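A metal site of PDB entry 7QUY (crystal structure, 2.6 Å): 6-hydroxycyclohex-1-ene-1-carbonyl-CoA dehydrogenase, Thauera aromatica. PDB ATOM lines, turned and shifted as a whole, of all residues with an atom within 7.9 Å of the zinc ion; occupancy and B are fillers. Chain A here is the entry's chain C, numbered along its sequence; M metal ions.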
ATOM      1  N   MET A  92      -4.435   2.781 -24.747  1.00  0.00           N
ATOM      2  CA  MET A  92      -3.354   2.370 -25.688  1.00  0.00           C
ATOM      3  C   MET A  92      -2.074   3.160 -25.413  1.00  0.00           C
ATOM      4  O   MET A  92      -1.994   4.345 -25.712  1.00  0.00           O
ATOM      5  CB  MET A  92      -3.787   2.579 -27.146  1.00  0.00           C
ATOM      6  CG  MET A  92      -5.019   1.808 -27.500  1.00  0.00           C
ATOM      7  SD  MET A  92      -6.052   2.578 -28.788  1.00  0.00           S
ATOM      8  CE  MET A  92      -5.535   1.616 -30.214  1.00  0.00           C
ATOM      9  N   PRO A  93      -1.065   2.538 -24.773  1.00  0.00           N
ATOM     10  CA  PRO A  93       0.260   3.134 -24.612  1.00  0.00           C
ATOM     11  C   PRO A  93       0.958   3.402 -25.951  1.00  0.00           C
ATOM     12  O   PRO A  93       0.609   2.683 -26.894  1.00  0.00           O
ATOM     13  CB  PRO A  93       1.044   2.066 -23.843  1.00  0.00           C
ATOM     14  CG  PRO A  93      -0.004   1.248 -23.146  1.00  0.00           C
ATOM     15  CD  PRO A  93      -1.174   1.245 -24.091  1.00  0.00           C
ATOM     16  N   CYS A  94       2.006   4.296 -25.937  1.00  0.00           N
ATOM     17  CA  CYS A  94       2.894   4.729 -27.089  1.00  0.00           C
ATOM     18  C   CYS A  94       3.553   3.536 -27.756  1.00  0.00           C
ATOM     19  O   CYS A  94       3.672   3.532 -28.990  1.00  0.00           O
ATOM     20  CB  CYS A  94       3.978   5.766 -26.681  1.00  0.00           C
ATOM     21  SG  CYS A  94       5.603   5.331 -25.936  1.00  0.00           S
ATOM     22  N   GLY A  95       3.910   2.550 -26.969  1.00  0.00           N
ATOM     23  CA  GLY A  95       4.648   1.343 -27.416  1.00  0.00           C
ATOM     24  C   GLY A  95       6.113   1.651 -27.726  1.00  0.00           C
ATOM     25  O   GLY A  95       6.841   0.689 -28.040  1.00  0.00           O
ATOM     26  N   THR A  96       6.548   2.911 -27.670  1.00  0.00           N
ATOM     27  CA  THR A  96       7.860   3.362 -28.223  1.00  0.00           C
ATOM     28  C   THR A  96       8.705   4.120 -27.185  1.00  0.00           C
ATOM     29  O   THR A  96       9.928   4.218 -27.438  1.00  0.00           O
ATOM     30  CB  THR A  96       7.673   4.235 -29.471  1.00  0.00           C
ATOM     31  OG1 THR A  96       7.124   5.486 -29.056  1.00  0.00           O
ATOM     32  CG2 THR A  96       6.793   3.599 -30.523  1.00  0.00           C
ATOM     33  N   CYS A  97       8.128   4.646 -26.084  1.00  0.00           N
ATOM     34  CA  CYS A  97       8.953   5.367 -25.080  1.00  0.00           C
ATOM     35  C   CYS A  97       9.657   4.379 -24.152  1.00  0.00           C
ATOM     36  O   CYS A  97       9.356   3.176 -24.205  1.00  0.00           O
ATOM     37  CB  CYS A  97       8.213   6.292 -24.111  1.00  0.00           C
ATOM     38  SG  CYS A  97       7.389   5.397 -22.871  1.00  0.00           S
ATOM     39  N   GLU A  98      10.493   4.921 -23.270  1.00  0.00           N
ATOM     40  CA  GLU A  98      11.244   4.167 -22.231  1.00  0.00           C
ATOM     41  C   GLU A  98      10.269   3.449 -21.286  1.00  0.00           C
ATOM     42  O   GLU A  98      10.558   2.291 -20.941  1.00  0.00           O
ATOM     43  CB  GLU A  98      12.196   5.115 -21.504  1.00  0.00           C
ATOM     44  CG  GLU A  98      13.090   4.392 -20.510  1.00  0.00           C
ATOM     45  CD  GLU A  98      12.536   4.296 -19.098  1.00  0.00           C
ATOM     46  OE1 GLU A  98      11.781   5.221 -18.703  1.00  0.00           O
ATOM     47  OE2 GLU A  98      12.858   3.306 -18.410  1.00  0.00           O
ATOM     48  N   LEU A  99       9.184   4.093 -20.850  1.00  0.00           N
ATOM     49  CA  LEU A  99       8.180   3.479 -19.933  1.00  0.00           C
ATOM     50  C   LEU A  99       7.537   2.265 -20.615  1.00  0.00           C
ATOM     51  O   LEU A  99       7.541   1.173 -20.025  1.00  0.00           O
ATOM     52  CB  LEU A  99       7.110   4.506 -19.537  1.00  0.00           C
ATOM     53  CG  LEU A  99       7.596   5.671 -18.674  1.00  0.00           C
ATOM     54  CD1 LEU A  99       6.462   6.626 -18.393  1.00  0.00           C
ATOM     55  CD2 LEU A  99       8.185   5.156 -17.366  1.00  0.00           C
ATOM     56  N   CYS A 100       7.019   2.445 -21.837  1.00  0.00           N
ATOM     57  CA  CYS A 100       6.329   1.396 -22.621  1.00  0.00           C
ATOM     58  C   CYS A 100       7.334   0.251 -22.861  1.00  0.00           C
ATOM     59  O   CYS A 100       6.993  -0.938 -22.646  1.00  0.00           O
ATOM     60  CB  CYS A 100       5.786   1.963 -23.947  1.00  0.00           C
ATOM     61  SG  CYS A 100       4.418   3.131 -23.920  1.00  0.00           S
ATOM     62  N   THR A 101       8.587   0.584 -23.179  1.00  0.00           N
ATOM     63  CA  THR A 101       9.616  -0.387 -23.664  1.00  0.00           C
ATOM     64  C   THR A 101      10.272  -1.101 -22.464  1.00  0.00           C
ATOM     65  O   THR A 101      10.960  -2.114 -22.682  1.00  0.00           O
ATOM     66  CB  THR A 101      10.607   0.319 -24.586  1.00  0.00           C
ATOM     67  OG1 THR A 101      10.979  -0.622 -25.595  1.00  0.00           O
ATOM     68  CG2 THR A 101      11.827   0.872 -23.884  1.00  0.00           C
ATOM     69  N   HIS A 104       6.432  -0.751 -18.439  1.00  0.00           N
ATOM     70  CA  HIS A 104       5.598   0.205 -17.642  1.00  0.00           C
ATOM     71  C   HIS A 104       4.577   0.940 -18.523  1.00  0.00           C
ATOM     72  O   HIS A 104       4.224   2.109 -18.175  1.00  0.00           O
ATOM     73  CB  HIS A 104       6.491   1.205 -16.897  1.00  0.00           C
ATOM     74  CG  HIS A 104       7.318   0.572 -15.831  1.00  0.00           C
ATOM     75  ND1 HIS A 104       8.548  -0.014 -16.094  1.00  0.00           N
ATOM     76  CD2 HIS A 104       7.103   0.428 -14.502  1.00  0.00           C
ATOM     77  CE1 HIS A 104       9.054  -0.496 -14.980  1.00  0.00           C
ATOM     78  NE2 HIS A 104       8.190  -0.232 -13.995  1.00  0.00           N
ATOM     79  N   GLY A 105       4.085   0.285 -19.583  1.00  0.00           N
ATOM     80  CA  GLY A 105       3.021   0.818 -20.465  1.00  0.00           C
ATOM     81  C   GLY A 105       1.813   1.406 -19.713  1.00  0.00           C
ATOM     82  O   GLY A 105       1.209   2.362 -20.228  1.00  0.00           O
ATOM     83  N   THR A 106       1.419   0.861 -18.562  1.00  0.00           N
ATOM     84  CA  THR A 106       0.230   1.353 -17.811  1.00  0.00           C
ATOM     85  C   THR A 106       0.422   2.809 -17.384  1.00  0.00           C
ATOM     86  O   THR A 106      -0.592   3.461 -17.105  1.00  0.00           O
ATOM     87  CB  THR A 106      -0.094   0.471 -16.602  1.00  0.00           C
ATOM     88  OG1 THR A 106       1.110   0.175 -15.893  1.00  0.00           O
ATOM     89  CG2 THR A 106      -0.791  -0.809 -16.996  1.00  0.00           C
ATOM     90  N   ILE A 107       1.662   3.312 -17.338  1.00  0.00           N
ATOM     91  CA  ILE A 107       1.932   4.727 -16.937  1.00  0.00           C
ATOM     92  C   ILE A 107       2.571   5.510 -18.090  1.00  0.00           C
ATOM     93  O   ILE A 107       3.120   6.594 -17.782  1.00  0.00           O
ATOM     94  CB  ILE A 107       2.765   4.795 -15.641  1.00  0.00           C
ATOM     95  CG1 ILE A 107       4.050   3.961 -15.718  1.00  0.00           C
ATOM     96  CG2 ILE A 107       1.888   4.421 -14.450  1.00  0.00           C
ATOM     97  CD1 ILE A 107       5.049   4.230 -14.620  1.00  0.00           C
ATOM     98  N   CYS A 108       2.457   5.042 -19.348  1.00  0.00           N
ATOM     99  CA  CYS A 108       2.847   5.827 -20.550  1.00  0.00           C
ATOM    100  C   CYS A 108       2.208   7.207 -20.378  1.00  0.00           C
ATOM    101  O   CYS A 108       1.043   7.284 -19.932  1.00  0.00           O
ATOM    102  CB  CYS A 108       2.445   5.194 -21.881  1.00  0.00           C
ATOM    103  SG  CYS A 108       3.053   6.180 -23.197  1.00  0.00           S
ATOM    104  N   ARG A 109       2.959   8.258 -20.670  1.00  0.00           N
ATOM    105  CA  ARG A 109       2.442   9.638 -20.505  1.00  0.00           C
ATOM    106  C   ARG A 109       1.598   9.981 -21.751  1.00  0.00           C
ATOM    107  O   ARG A 109       0.833  10.969 -21.722  1.00  0.00           O
ATOM    108  CB  ARG A 109       3.576  10.641 -20.329  1.00  0.00           C
ATOM    109  CG  ARG A 109       4.340  10.545 -19.021  1.00  0.00           C
ATOM    110  CD  ARG A 109       5.287  11.710 -18.862  1.00  0.00           C
ATOM    111  NE  ARG A 109       5.926  11.697 -17.553  1.00  0.00           N
ATOM    112  CZ  ARG A 109       7.083  11.094 -17.255  1.00  0.00           C
ATOM    113  NH1 ARG A 109       7.771  10.468 -18.194  1.00  0.00           N
ATOM    114  NH2 ARG A 109       7.548  11.134 -16.019  1.00  0.00           N
ATOM    115  N   ASP A 110       1.745   9.167 -22.810  1.00  0.00           N
ATOM    116  CA  ASP A 110       1.158   9.344 -24.173  1.00  0.00           C
ATOM    117  C   ASP A 110       0.178   8.199 -24.461  1.00  0.00           C
ATOM    118  O   ASP A 110       0.121   7.769 -25.616  1.00  0.00           O
ATOM    119  CB  ASP A 110       2.232   9.327 -25.267  1.00  0.00           C
ATOM    120  CG  ASP A 110       3.532  10.024 -24.936  1.00  0.00           C
ATOM    121  OD1 ASP A 110       3.511  11.265 -24.736  1.00  0.00           O
ATOM    122  OD2 ASP A 110       4.569   9.323 -24.880  1.00  0.00           O
ATOM    123  N   GLN A 111      -0.563   7.720 -23.455  1.00  0.00           N
ATOM    124  CA  GLN A 111      -1.597   6.671 -23.608  1.00  0.00           C
ATOM    125  C   GLN A 111      -2.891   7.354 -24.073  1.00  0.00           C
ATOM    126  O   GLN A 111      -3.142   8.495 -23.638  1.00  0.00           O
ATOM    127  CB  GLN A 111      -1.766   5.831 -22.339  1.00  0.00           C
ATOM    128  CG  GLN A 111      -2.214   6.601 -21.099  1.00  0.00           C
ATOM    129  CD  GLN A 111      -2.286   5.755 -19.852  1.00  0.00           C
ATOM    130  OE1 GLN A 111      -3.265   5.784 -19.106  1.00  0.00           O
ATOM    131  NE2 GLN A 111      -1.238   4.992 -19.592  1.00  0.00           N
ATOM    132  N   ARG A 131      -1.744   0.404 -33.316  1.00  0.00           N
ATOM    133  CA  ARG A 131      -0.834  -0.268 -32.347  1.00  0.00           C
ATOM    134  C   ARG A 131      -1.708  -0.793 -31.188  1.00  0.00           C
ATOM    135  O   ARG A 131      -2.494   0.001 -30.586  1.00  0.00           O
ATOM    136  CB  ARG A 131       0.373   0.606 -31.970  1.00  0.00           C
ATOM    137  CG  ARG A 131       0.240   1.500 -30.740  1.00  0.00           C
ATOM    138  CD  ARG A 131      -0.870   2.522 -30.903  1.00  0.00           C
ATOM    139  NE  ARG A 131      -0.926   3.485 -29.812  1.00  0.00           N
ATOM    140  CZ  ARG A 131      -0.430   4.724 -29.839  1.00  0.00           C
ATOM    141  NH1 ARG A 131       0.176   5.183 -30.921  1.00  0.00           N
ATOM    142  NH2 ARG A 131      -0.552   5.503 -28.778  1.00  0.00           N
HETATM  143 ZN    ZN M   1       5.159   5.308 -23.459  1.00  0.00          ZN
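The side-chain sulfur of Cys 94 lies close to the backbone NH of Thr 96, at 3.1 Å.
The side-chain sulfur (SG) of Cys 97 sits close to the backbone NH (N) of Leu 99 (3.0 Å).
The backbone NH of Asp 110 sits close to the side-chain sulfur of Cys 108 (3.3 Å).
The side-chain amide nitrogen (NE2) of Gln 111 lies within hydrogen-bond range of the backbone carbonyl oxygen (O) of Cys 108 (3.3 Å).
The side-chain sulfur of Cys 100 sits close to the backbone NH of Gly 95, at 3.1 Å.
Within 4 Å of the zinc ion: Cys 94, Cys 97, Cys 100 and Cys 108.
SG of Cys 108 is bound to the zinc ion.
The side-chain sulfur (SG) of Cys 97 binds the zinc ion.
SG of Cys 100 is bound to the zinc ion, 2.3 Å away.
SG of Cys 94 binds the zinc ion (2.5 Å).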
